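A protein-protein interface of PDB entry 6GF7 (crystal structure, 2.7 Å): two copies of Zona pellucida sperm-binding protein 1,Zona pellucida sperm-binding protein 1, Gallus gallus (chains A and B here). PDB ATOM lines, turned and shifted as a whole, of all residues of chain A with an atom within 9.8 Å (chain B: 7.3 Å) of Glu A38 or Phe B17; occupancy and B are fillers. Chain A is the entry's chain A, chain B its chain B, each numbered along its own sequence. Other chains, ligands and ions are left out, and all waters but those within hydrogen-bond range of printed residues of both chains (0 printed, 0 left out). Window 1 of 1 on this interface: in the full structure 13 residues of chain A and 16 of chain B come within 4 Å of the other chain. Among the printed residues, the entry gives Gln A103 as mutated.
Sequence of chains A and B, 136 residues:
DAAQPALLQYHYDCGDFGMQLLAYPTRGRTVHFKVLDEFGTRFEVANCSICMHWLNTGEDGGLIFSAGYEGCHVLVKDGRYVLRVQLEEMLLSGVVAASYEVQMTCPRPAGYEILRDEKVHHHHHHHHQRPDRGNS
O of Leu A75 is in hydrogen-bond range of N of Val A82, 2.8 Å away.
The side-chain carboxylate (OD1) of Asp A37 sits at hydrogen-bond distance from the backbone NH (N) of Thr A41 (2.7 Å).
O of Gly B18 lies within hydrogen-bond range of OH of Tyr B69.
OD1 of Asp A37 sits close to N of Phe A39.
N of Tyr B69 sits at hydrogen-bond distance from O of Phe B17, at 3.0 Å.
The backbone carbonyl oxygen (O) of Met B52 is in hydrogen-bond range of the backbone NH (N) of Gly B68.
Hydrophobic or aromatic side chains of chain A within 4 Å of the printed part of chain B: Phe A39 and Leu A75.
Among the printed residues, 13 pairs touch across the chains.
OG1 of Thr A41 sits at hydrogen-bond distance from OE1 of Gln B20 (3.0 Å).
N of Asp B16 lies within hydrogen-bond range of OE1 of Glu A38.
The backbone NH (N) of Phe B17 is in hydrogen-bond range of the side-chain carboxylate (OE2) of Glu A38.
N of Gly B18 lies within hydrogen-bond range of OE2 of Glu A38.
Of chain B, only Gly B15 (3.5 Å), Asp B16 (2.8 Å), Phe B17 (2.8 Å) and Gly B18 (3.1 Å) come within 4 Å of Glu A38.
Phe B17 touches just these residues of chain A: Glu A38 (2.8 Å), Leu A75 (3.6 Å) and Lys A77 (3.8 Å).
Of chain A, only Glu A38 (2.8 Å) comes within 4 Å of Asp B16.
Gly B18 touches just these residues of chain A: Glu A38 and Phe A39.
No residue of chain A comes within 4 Å of Gly B68.
Of the printed residues of chain B, Lys A77 touches Phe B17.
Of the printed residues of chain A, Cys B14 touches Phe A39.
Of the printed residues of chain A, Gln B20 touches Phe A39 and Thr A41.
Of the printed residues of chain B, Leu A75 touches Phe B17.
Tyr B81 touches none of the printed residues of chain A.
His A73 touches none of the printed residues of chain B.
The nearest printed residue of chain B that does not touch Glu A38 is Met B19 (5.4 Å).
The nearest printed residue of chain B that does not touch Phe A39 is Asp B16 (5.3 Å).
OE2 of Glu A38 touches C of Gly B15, 3.5 Å away.
C of Cys B14 touches CZ of Phe A39, at 3.96 Å.
CZ of Phe A39 touches N of Gly B15, at 3.4 Å.
Gly B18 touches Phe A39 (O to CZ, 3.3 Å).
Phe A39 touches Met B19.
Gln B20 touches Phe A39.
Cys A72 touches Met B52 (SG to CG, 3.7 Å).
Leu A75 touches Phe B17.
CG of Lys A77 touches CZ of Phe B17, 3.8 Å away.
No position is printed for both chains.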
ATOM      1  N   VAL A  35      -5.337   6.639  -5.850  1.00  0.00           N
ATOM      2  CA  VAL A  35      -6.364   5.971  -5.063  1.00  0.00           C
ATOM      3  C   VAL A  35      -6.939   4.836  -5.889  1.00  0.00           C
ATOM      4  O   VAL A  35      -7.173   4.988  -7.093  1.00  0.00           O
ATOM      5  CB  VAL A  35      -7.468   6.964  -4.650  1.00  0.00           C
ATOM      6  CG1 VAL A  35      -8.563   6.248  -3.895  1.00  0.00           C
ATOM      7  CG2 VAL A  35      -6.890   8.077  -3.799  1.00  0.00           C
ATOM      8  N   LEU A  36      -7.177   3.698  -5.244  1.00  0.00           N
ATOM      9  CA  LEU A  36      -7.754   2.528  -5.893  1.00  0.00           C
ATOM     10  C   LEU A  36      -9.170   2.338  -5.370  1.00  0.00           C
ATOM     11  O   LEU A  36      -9.374   2.218  -4.158  1.00  0.00           O
ATOM     12  CB  LEU A  36      -6.915   1.282  -5.620  1.00  0.00           C
ATOM     13  CG  LEU A  36      -5.417   1.416  -5.872  1.00  0.00           C
ATOM     14  CD1 LEU A  36      -4.662   0.162  -5.439  1.00  0.00           C
ATOM     15  CD2 LEU A  36      -5.200   1.689  -7.333  1.00  0.00           C
ATOM     16  N   ASP A  37     -10.134   2.279  -6.281  1.00  0.00           N
ATOM     17  CA  ASP A  37     -11.504   1.940  -5.932  1.00  0.00           C
ATOM     18  C   ASP A  37     -11.710   0.431  -6.029  1.00  0.00           C
ATOM     19  O   ASP A  37     -10.829  -0.316  -6.458  1.00  0.00           O
ATOM     20  CB  ASP A  37     -12.496   2.693  -6.828  1.00  0.00           C
ATOM     21  CG  ASP A  37     -12.538   2.168  -8.265  1.00  0.00           C
ATOM     22  OD1 ASP A  37     -11.677   1.353  -8.657  1.00  0.00           O
ATOM     23  OD2 ASP A  37     -13.446   2.588  -9.018  1.00  0.00           O
ATOM     24  N   GLU A  38     -12.900  -0.015  -5.623  1.00  0.00           N
ATOM     25  CA  GLU A  38     -13.193  -1.443  -5.599  1.00  0.00           C
ATOM     26  C   GLU A  38     -13.206  -2.081  -6.983  1.00  0.00           C
ATOM     27  O   GLU A  38     -13.202  -3.312  -7.070  1.00  0.00           O
ATOM     28  CB  GLU A  38     -14.534  -1.690  -4.909  1.00  0.00           C
ATOM     29  CG  GLU A  38     -15.714  -1.059  -5.615  1.00  0.00           C
ATOM     30  CD  GLU A  38     -17.033  -1.388  -4.941  1.00  0.00           C
ATOM     31  OE1 GLU A  38     -17.105  -2.421  -4.239  1.00  0.00           O
ATOM     32  OE2 GLU A  38     -17.989  -0.598  -5.093  1.00  0.00           O
ATOM     33  N   PHE A  39     -13.213  -1.294  -8.057  1.00  0.00           N
ATOM     34  CA  PHE A  39     -13.160  -1.831  -9.410  1.00  0.00           C
ATOM     35  C   PHE A  39     -11.755  -1.816  -9.999  1.00  0.00           C
ATOM     36  O   PHE A  39     -11.597  -2.027 -11.206  1.00  0.00           O
ATOM     37  CB  PHE A  39     -14.102  -1.052 -10.324  1.00  0.00           C
ATOM     38  CG  PHE A  39     -15.532  -1.082  -9.881  1.00  0.00           C
ATOM     39  CD1 PHE A  39     -16.280  -2.242  -9.983  1.00  0.00           C
ATOM     40  CD2 PHE A  39     -16.133   0.056  -9.368  1.00  0.00           C
ATOM     41  CE1 PHE A  39     -17.601  -2.269  -9.577  1.00  0.00           C
ATOM     42  CE2 PHE A  39     -17.450   0.038  -8.960  1.00  0.00           C
ATOM     43  CZ  PHE A  39     -18.185  -1.124  -9.063  1.00  0.00           C
ATOM     44  N   GLY A  40     -10.736  -1.566  -9.183  1.00  0.00           N
ATOM     45  CA  GLY A  40      -9.368  -1.573  -9.646  1.00  0.00           C
ATOM     46  C   GLY A  40      -8.928  -0.308 -10.347  1.00  0.00           C
ATOM     47  O   GLY A  40      -7.749  -0.199 -10.710  1.00  0.00           O
ATOM     48  N   THR A  41      -9.827   0.650 -10.543  1.00  0.00           N
ATOM     49  CA  THR A  41      -9.477   1.909 -11.185  1.00  0.00           C
ATOM     50  C   THR A  41      -8.494   2.693 -10.321  1.00  0.00           C
ATOM     51  O   THR A  41      -8.539   2.643  -9.090  1.00  0.00           O
ATOM     52  CB  THR A  41     -10.732   2.748 -11.436  1.00  0.00           C
ATOM     53  OG1 THR A  41     -11.743   1.931 -12.035  1.00  0.00           O
ATOM     54  CG2 THR A  41     -10.422   3.895 -12.385  1.00  0.00           C
ATOM     55  N   ARG A  42      -7.600   3.425 -10.979  1.00  0.00           N
ATOM     56  CA  ARG A  42      -6.607   4.252 -10.306  1.00  0.00           C
ATOM     57  C   ARG A  42      -6.914   5.720 -10.558  1.00  0.00           C
ATOM     58  O   ARG A  42      -7.108   6.125 -11.708  1.00  0.00           O
ATOM     59  CB  ARG A  42      -5.195   3.907 -10.789  1.00  0.00           C
ATOM     60  CG  ARG A  42      -4.927   2.404 -10.806  1.00  0.00           C
ATOM     61  CD  ARG A  42      -3.535   2.059 -11.302  1.00  0.00           C
ATOM     62  NE  ARG A  42      -3.420   0.646 -11.663  1.00  0.00           N
ATOM     63  CZ  ARG A  42      -3.316  -0.353 -10.788  1.00  0.00           C
ATOM     64  NH1 ARG A  42      -3.310  -0.105  -9.483  1.00  0.00           N
ATOM     65  NH2 ARG A  42      -3.216  -1.604 -11.220  1.00  0.00           N
ATOM     66  N   PHE A  43      -7.035   6.499  -9.478  1.00  0.00           N
ATOM     67  CA  PHE A  43      -7.281   7.939  -9.561  1.00  0.00           C
ATOM     68  C   PHE A  43      -6.037   8.654  -9.049  1.00  0.00           C
ATOM     69  O   PHE A  43      -5.780   8.649  -7.841  1.00  0.00           O
ATOM     70  CB  PHE A  43      -8.494   8.334  -8.725  1.00  0.00           C
ATOM     71  CG  PHE A  43      -9.737   7.573  -9.061  1.00  0.00           C
ATOM     72  CD1 PHE A  43      -9.977   6.333  -8.491  1.00  0.00           C
ATOM     73  CD2 PHE A  43     -10.676   8.100  -9.931  1.00  0.00           C
ATOM     74  CE1 PHE A  43     -11.122   5.629  -8.792  1.00  0.00           C
ATOM     75  CE2 PHE A  43     -11.826   7.400 -10.231  1.00  0.00           C
ATOM     76  CZ  PHE A  43     -12.050   6.164  -9.661  1.00  0.00           C
ATOM     77  N   CYS A  72     -13.929  12.119  -0.578  1.00  0.00           N
ATOM     78  CA  CYS A  72     -14.882  11.399  -1.426  1.00  0.00           C
ATOM     79  C   CYS A  72     -14.489   9.941  -1.687  1.00  0.00           C
ATOM     80  O   CYS A  72     -15.375   9.091  -1.830  1.00  0.00           O
ATOM     81  CB  CYS A  72     -15.082  12.145  -2.743  1.00  0.00           C
ATOM     82  SG  CYS A  72     -16.309  13.471  -2.614  1.00  0.00           S
ATOM     83  N   HIS A  73     -13.191   9.626  -1.752  1.00  0.00           N
ATOM     84  CA  HIS A  73     -12.743   8.260  -2.027  1.00  0.00           C
ATOM     85  C   HIS A  73     -12.750   7.367  -0.791  1.00  0.00           C
ATOM     86  O   HIS A  73     -12.546   6.155  -0.909  1.00  0.00           O
ATOM     87  CB  HIS A  73     -11.335   8.287  -2.620  1.00  0.00           C
ATOM     88  CG  HIS A  73     -11.166   9.280  -3.726  1.00  0.00           C
ATOM     89  ND1 HIS A  73     -11.195   8.925  -5.057  1.00  0.00           N
ATOM     90  CD2 HIS A  73     -10.967  10.619  -3.699  1.00  0.00           C
ATOM     91  CE1 HIS A  73     -11.018  10.000  -5.802  1.00  0.00           C
ATOM     92  NE2 HIS A  73     -10.877  11.042  -5.003  1.00  0.00           N
ATOM     93  N   VAL A  74     -13.009   7.945   0.365  1.00  0.00           N
ATOM     94  CA  VAL A  74     -12.844   7.330   1.675  1.00  0.00           C
ATOM     95  C   VAL A  74     -14.124   6.583   2.024  1.00  0.00           C
ATOM     96  O   VAL A  74     -15.226   7.138   1.944  1.00  0.00           O
ATOM     97  CB  VAL A  74     -12.488   8.382   2.738  1.00  0.00           C
ATOM     98  CG1 VAL A  74     -12.332   7.723   4.100  1.00  0.00           C
ATOM     99  CG2 VAL A  74     -11.197   9.098   2.355  1.00  0.00           C
ATOM    100  N   LEU A  75     -13.984   5.311   2.376  1.00  0.00           N
ATOM    101  CA  LEU A  75     -15.100   4.442   2.702  1.00  0.00           C
ATOM    102  C   LEU A  75     -15.095   4.104   4.185  1.00  0.00           C
ATOM    103  O   LEU A  75     -14.058   4.150   4.854  1.00  0.00           O
ATOM    104  CB  LEU A  75     -15.028   3.146   1.889  1.00  0.00           C
ATOM    105  CG  LEU A  75     -15.034   3.269   0.367  1.00  0.00           C
ATOM    106  CD1 LEU A  75     -14.888   1.891  -0.270  1.00  0.00           C
ATOM    107  CD2 LEU A  75     -16.296   3.965  -0.111  1.00  0.00           C
ATOM    108  N   VAL A  76     -16.271   3.753   4.696  1.00  0.00           N
ATOM    109  CA  VAL A  76     -16.412   3.234   6.051  1.00  0.00           C
ATOM    110  C   VAL A  76     -16.589   1.727   5.948  1.00  0.00           C
ATOM    111  O   VAL A  76     -17.500   1.246   5.265  1.00  0.00           O
ATOM    112  CB  VAL A  76     -17.586   3.884   6.796  1.00  0.00           C
ATOM    113  CG1 VAL A  76     -17.685   3.306   8.187  1.00  0.00           C
ATOM    114  CG2 VAL A  76     -17.405   5.394   6.862  1.00  0.00           C
ATOM    115  N   LYS A  77     -15.691   0.981   6.589  1.00  0.00           N
ATOM    116  CA  LYS A  77     -15.716  -0.476   6.569  1.00  0.00           C
ATOM    117  C   LYS A  77     -15.370  -0.959   7.968  1.00  0.00           C
ATOM    118  O   LYS A  77     -14.312  -0.606   8.495  1.00  0.00           O
ATOM    119  CB  LYS A  77     -14.725  -1.024   5.535  1.00  0.00           C
ATOM    120  CG  LYS A  77     -15.072  -0.643   4.096  1.00  0.00           C
ATOM    121  CD  LYS A  77     -14.003  -1.072   3.100  1.00  0.00           C
ATOM    122  CE  LYS A  77     -13.940  -2.583   2.937  1.00  0.00           C
ATOM    123  NZ  LYS A  77     -12.934  -2.991   1.910  1.00  0.00           N
ATOM    124  N   ASP A  78     -16.273  -1.740   8.571  1.00  0.00           N
ATOM    125  CA  ASP A  78     -16.115  -2.217   9.950  1.00  0.00           C
ATOM    126  C   ASP A  78     -15.861  -1.057  10.910  1.00  0.00           C
ATOM    127  O   ASP A  78     -15.007  -1.131  11.798  1.00  0.00           O
ATOM    128  CB  ASP A  78     -15.002  -3.259  10.060  1.00  0.00           C
ATOM    129  CG  ASP A  78     -15.068  -4.048  11.359  1.00  0.00           C
ATOM    130  OD1 ASP A  78     -16.125  -4.013  12.025  1.00  0.00           O
ATOM    131  OD2 ASP A  78     -14.057  -4.685  11.724  1.00  0.00           O
ATOM    132  N   GLY A  79     -16.610   0.026  10.732  1.00  0.00           N
ATOM    133  CA  GLY A  79     -16.476   1.158  11.626  1.00  0.00           C
ATOM    134  C   GLY A  79     -15.130   1.836  11.544  1.00  0.00           C
ATOM    135  O   GLY A  79     -14.692   2.449  12.523  1.00  0.00           O
ATOM    136  N   ARG A  80     -14.459   1.749  10.397  1.00  0.00           N
ATOM    137  CA  ARG A  80     -13.163   2.381  10.214  1.00  0.00           C
ATOM    138  C   ARG A  80     -13.099   3.040   8.843  1.00  0.00           C
ATOM    139  O   ARG A  80     -13.626   2.507   7.862  1.00  0.00           O
ATOM    140  CB  ARG A  80     -12.036   1.351  10.370  1.00  0.00           C
ATOM    141  CG  ARG A  80     -11.899   0.810  11.783  1.00  0.00           C
ATOM    142  CD  ARG A  80     -10.728  -0.139  11.920  1.00  0.00           C
ATOM    143  NE  ARG A  80     -10.405  -0.391  13.320  1.00  0.00           N
ATOM    144  CZ  ARG A  80     -11.010  -1.301  14.076  1.00  0.00           C
ATOM    145  NH1 ARG A  80     -11.979  -2.051  13.567  1.00  0.00           N
ATOM    146  NH2 ARG A  80     -10.650  -1.456  15.342  1.00  0.00           N
ATOM    147  N   VAL A  82     -11.347   3.775   5.497  1.00  0.00           N
ATOM    148  CA  VAL A  82     -10.439   2.943   4.717  1.00  0.00           C
ATOM    149  C   VAL A  82     -10.173   3.610   3.378  1.00  0.00           C
ATOM    150  O   VAL A  82     -11.109   4.031   2.688  1.00  0.00           O
ATOM    151  CB  VAL A  82     -10.999   1.522   4.505  1.00  0.00           C
ATOM    152  CG1 VAL A  82     -10.034   0.683   3.676  1.00  0.00           C
ATOM    153  CG2 VAL A  82     -11.269   0.851   5.840  1.00  0.00           C
ATOM    154  N   LEU A  83      -8.897   3.703   3.014  1.00  0.00           N
ATOM    155  CA  LEU A  83      -8.489   4.210   1.712  1.00  0.00           C
ATOM    156  C   LEU A  83      -7.350   3.340   1.209  1.00  0.00           C
ATOM    157  O   LEU A  83      -6.347   3.162   1.910  1.00  0.00           O
ATOM    158  CB  LEU A  83      -8.059   5.677   1.794  1.00  0.00           C
ATOM    159  CG  LEU A  83      -7.869   6.410   0.470  1.00  0.00           C
ATOM    160  CD1 LEU A  83      -9.174   6.424  -0.283  1.00  0.00           C
ATOM    161  CD2 LEU A  83      -7.393   7.837   0.717  1.00  0.00           C
ATOM    162  N   ARG A  84      -7.503   2.800   0.004  1.00  0.00           N
ATOM    163  CA  ARG A  84      -6.473   1.966  -0.597  1.00  0.00           C
ATOM    164  C   ARG A  84      -5.694   2.831  -1.579  1.00  0.00           C
ATOM    165  O   ARG A  84      -6.279   3.417  -2.496  1.00  0.00           O
ATOM    166  CB  ARG A  84      -7.086   0.750  -1.288  1.00  0.00           C
ATOM    167  CG  ARG A  84      -6.066  -0.255  -1.790  1.00  0.00           C
ATOM    168  CD  ARG A  84      -6.740  -1.394  -2.549  1.00  0.00           C
ATOM    169  NE  ARG A  84      -7.581  -2.208  -1.677  1.00  0.00           N
ATOM    170  CZ  ARG A  84      -7.117  -3.144  -0.855  1.00  0.00           C
ATOM    171  NH1 ARG A  84      -5.813  -3.382  -0.782  1.00  0.00           N
ATOM    172  NH2 ARG A  84      -7.954  -3.840  -0.095  1.00  0.00           N
ATOM    173  N   GLN A 103      -3.017   0.014   2.344  1.00  0.00           N
ATOM    174  CA  GLN A 103      -4.406   0.210   2.737  1.00  0.00           C
ATOM    175  C   GLN A 103      -4.397   0.984   4.042  1.00  0.00           C
ATOM    176  O   GLN A 103      -4.003   0.455   5.085  1.00  0.00           O
ATOM    177  CB  GLN A 103      -5.150  -1.113   2.897  1.00  0.00           C
ATOM    178  CG  GLN A 103      -6.646  -0.926   3.114  1.00  0.00           C
ATOM    179  CD  GLN A 103      -7.400  -2.232   3.237  1.00  0.00           C
ATOM    180  OE1 GLN A 103      -8.476  -2.391   2.659  1.00  0.00           O
ATOM    181  NE2 GLN A 103      -6.852  -3.169   4.001  1.00  0.00           N
ATOM    182  N   CYS B  14     -22.004  -3.304 -11.029  1.00  0.00           N
ATOM    183  CA  CYS B  14     -22.418  -2.861  -9.706  1.00  0.00           C
ATOM    184  C   CYS B  14     -21.419  -3.373  -8.681  1.00  0.00           C
ATOM    185  O   CYS B  14     -20.998  -4.534  -8.739  1.00  0.00           O
ATOM    186  CB  CYS B  14     -23.824  -3.349  -9.362  1.00  0.00           C
ATOM    187  SG  CYS B  14     -25.105  -2.762 -10.486  1.00  0.00           S
ATOM    188  N   GLY B  15     -21.010  -2.501  -7.776  1.00  0.00           N
ATOM    189  CA  GLY B  15     -20.088  -2.915  -6.745  1.00  0.00           C
ATOM    190  C   GLY B  15     -20.716  -2.813  -5.377  1.00  0.00           C
ATOM    191  O   GLY B  15     -21.938  -2.708  -5.246  1.00  0.00           O
ATOM    192  N   ASP B  16     -19.880  -2.800  -4.348  1.00  0.00           N
ATOM    193  CA  ASP B  16     -20.389  -2.746  -2.987  1.00  0.00           C
ATOM    194  C   ASP B  16     -20.703  -1.317  -2.570  1.00  0.00           C
ATOM    195  O   ASP B  16     -21.670  -1.079  -1.836  1.00  0.00           O
ATOM    196  CB  ASP B  16     -19.384  -3.380  -2.033  1.00  0.00           C
ATOM    197  CG  ASP B  16     -19.247  -4.869  -2.252  1.00  0.00           C
ATOM    198  OD1 ASP B  16     -20.166  -5.460  -2.862  1.00  0.00           O
ATOM    199  OD2 ASP B  16     -18.224  -5.446  -1.828  1.00  0.00           O
ATOM    200  N   PHE B  17     -19.884  -0.358  -3.003  1.00  0.00           N
ATOM    201  CA  PHE B  17     -20.062   1.030  -2.621  1.00  0.00           C
ATOM    202  C   PHE B  17     -20.376   1.954  -3.785  1.00  0.00           C
ATOM    203  O   PHE B  17     -20.613   3.144  -3.560  1.00  0.00           O
ATOM    204  CB  PHE B  17     -18.803   1.519  -1.905  1.00  0.00           C
ATOM    205  CG  PHE B  17     -18.425   0.662  -0.748  1.00  0.00           C
ATOM    206  CD1 PHE B  17     -18.972   0.882   0.502  1.00  0.00           C
ATOM    207  CD2 PHE B  17     -17.545  -0.396  -0.924  1.00  0.00           C
ATOM    208  CE1 PHE B  17     -18.629   0.077   1.568  1.00  0.00           C
ATOM    209  CE2 PHE B  17     -17.197  -1.203   0.136  1.00  0.00           C
ATOM    210  CZ  PHE B  17     -17.739  -0.968   1.385  1.00  0.00           C
ATOM    211  N   GLY B  18     -20.373   1.452  -5.015  1.00  0.00           N
ATOM    212  CA  GLY B  18     -20.663   2.295  -6.158  1.00  0.00           C
ATOM    213  C   GLY B  18     -20.825   1.457  -7.407  1.00  0.00           C
ATOM    214  O   GLY B  18     -20.712   0.229  -7.383  1.00  0.00           O
ATOM    215  N   MET B  19     -21.067   2.148  -8.514  1.00  0.00           N
ATOM    216  CA  MET B  19     -21.233   1.507  -9.805  1.00  0.00           C
ATOM    217  C   MET B  19     -20.220   2.079 -10.785  1.00  0.00           C
ATOM    218  O   MET B  19     -19.784   3.225 -10.655  1.00  0.00           O
ATOM    219  CB  MET B  19     -22.644   1.719 -10.356  1.00  0.00           C
ATOM    220  CG  MET B  19     -23.066   3.180 -10.348  1.00  0.00           C
ATOM    221  SD  MET B  19     -24.826   3.474 -10.648  1.00  0.00           S
ATOM    222  CE  MET B  19     -25.576   2.993  -9.100  1.00  0.00           C
ATOM    223  N   GLN B  20     -19.851   1.263 -11.766  1.00  0.00           N
ATOM    224  CA  GLN B  20     -18.864   1.620 -12.772  1.00  0.00           C
ATOM    225  C   GLN B  20     -19.451   1.368 -14.151  1.00  0.00           C
ATOM    226  O   GLN B  20     -20.038   0.310 -14.384  1.00  0.00           O
ATOM    227  CB  GLN B  20     -17.588   0.801 -12.572  1.00  0.00           C
ATOM    228  CG  GLN B  20     -16.646   0.834 -13.735  1.00  0.00           C
ATOM    229  CD  GLN B  20     -15.338   0.165 -13.416  1.00  0.00           C
ATOM    230  OE1 GLN B  20     -14.446   0.776 -12.826  1.00  0.00           O
ATOM    231  NE2 GLN B  20     -15.213  -1.103 -13.793  1.00  0.00           N
ATOM    232  N   MET B  52     -19.202  12.833  -5.989  1.00  0.00           N
ATOM    233  CA  MET B  52     -18.735  11.444  -5.961  1.00  0.00           C
ATOM    234  C   MET B  52     -18.976  10.739  -7.298  1.00  0.00           C
ATOM    235  O   MET B  52     -19.513   9.630  -7.353  1.00  0.00           O
ATOM    236  CB  MET B  52     -19.388  10.667  -4.813  1.00  0.00           C
ATOM    237  CG  MET B  52     -18.994  11.123  -3.422  1.00  0.00           C
ATOM    238  SD  MET B  52     -19.965  10.289  -2.148  1.00  0.00           S
ATOM    239  CE  MET B  52     -19.503   8.576  -2.407  1.00  0.00           C
ATOM    240  N   ALA B  67     -19.340   6.083 -10.046  1.00  0.00           N
ATOM    241  CA  ALA B  67     -20.330   6.820  -9.270  1.00  0.00           C
ATOM    242  C   ALA B  67     -20.569   6.105  -7.949  1.00  0.00           C
ATOM    243  O   ALA B  67     -20.898   4.915  -7.940  1.00  0.00           O
ATOM    244  CB  ALA B  67     -21.640   6.965 -10.045  1.00  0.00           C
ATOM    245  N   GLY B  68     -20.393   6.819  -6.839  1.00  0.00           N
ATOM    246  CA  GLY B  68     -20.724   6.252  -5.542  1.00  0.00           C
ATOM    247  C   GLY B  68     -22.229   6.168  -5.335  1.00  0.00           C
ATOM    248  O   GLY B  68     -22.988   7.033  -5.773  1.00  0.00           O
ATOM    249  N   TYR B  69     -22.661   5.104  -4.650  1.00  0.00           N
ATOM    250  CA  TYR B  69     -24.089   4.915  -4.393  1.00  0.00           C
ATOM    251  C   TYR B  69     -24.688   6.080  -3.613  1.00  0.00           C
ATOM    252  O   TYR B  69     -25.882   6.368  -3.753  1.00  0.00           O
ATOM    253  CB  TYR B  69     -24.334   3.606  -3.638  1.00  0.00           C
ATOM    254  CG  TYR B  69     -24.114   2.345  -4.451  1.00  0.00           C
ATOM    255  CD1 TYR B  69     -24.529   2.258  -5.769  1.00  0.00           C
ATOM    256  CD2 TYR B  69     -23.514   1.229  -3.881  1.00  0.00           C
ATOM    257  CE1 TYR B  69     -24.331   1.099  -6.503  1.00  0.00           C
ATOM    258  CE2 TYR B  69     -23.313   0.073  -4.602  1.00  0.00           C
ATOM    259  CZ  TYR B  69     -23.722   0.011  -5.912  1.00  0.00           C
ATOM    260  OH  TYR B  69     -23.519  -1.145  -6.630  1.00  0.00           O
ATOM    261  N   GLU B  70     -23.890   6.754  -2.782  1.00  0.00           N
ATOM    262  CA  GLU B  70     -24.367   7.889  -2.003  1.00  0.00           C
ATOM    263  C   GLU B  70     -24.060   9.229  -2.666  1.00  0.00           C
ATOM    264  O   GLU B  70     -24.007  10.255  -1.979  1.00  0.00           O
ATOM    265  CB  GLU B  70     -23.786   7.847  -0.591  1.00  0.00           C
ATOM    266  CG  GLU B  70     -24.338   6.706   0.253  1.00  0.00           C
ATOM    267  CD  GLU B  70     -23.923   6.796   1.709  1.00  0.00           C
ATOM    268  OE1 GLU B  70     -22.730   6.574   2.009  1.00  0.00           O
ATOM    269  OE2 GLU B  70     -24.795   7.092   2.554  1.00  0.00           O
ATOM    270  N   GLY B  71     -23.879   9.243  -3.984  1.00  0.00           N
ATOM    271  CA  GLY B  71     -23.588  10.461  -4.707  1.00  0.00           C
ATOM    272  C   GLY B  71     -24.812  11.337  -4.908  1.00  0.00           C
ATOM    273  O   GLY B  71     -25.867  11.152  -4.300  1.00  0.00           O
ATOM    274  N   TYR B  81     -30.667   1.063  -6.284  1.00  0.00           N
ATOM    275  CA  TYR B  81     -29.970   2.249  -6.762  1.00  0.00           C
ATOM    276  C   TYR B  81     -30.117   2.367  -8.273  1.00  0.00           C
ATOM    277  O   TYR B  81     -29.918   1.392  -9.003  1.00  0.00           O
ATOM    278  CB  TYR B  81     -28.487   2.200  -6.399  1.00  0.00           C
ATOM    279  CG  TYR B  81     -28.168   2.206  -4.922  1.00  0.00           C
ATOM    280  CD1 TYR B  81     -28.500   3.296  -4.129  1.00  0.00           C
ATOM    281  CD2 TYR B  81     -27.476   1.153  -4.333  1.00  0.00           C
ATOM    282  CE1 TYR B  81     -28.186   3.323  -2.784  1.00  0.00           C
ATOM    283  CE2 TYR B  81     -27.156   1.172  -2.986  1.00  0.00           C
ATOM    284  CZ  TYR B  81     -27.512   2.262  -2.216  1.00  0.00           C
ATOM    285  OH  TYR B  81     -27.200   2.297  -0.873  1.00  0.00           O
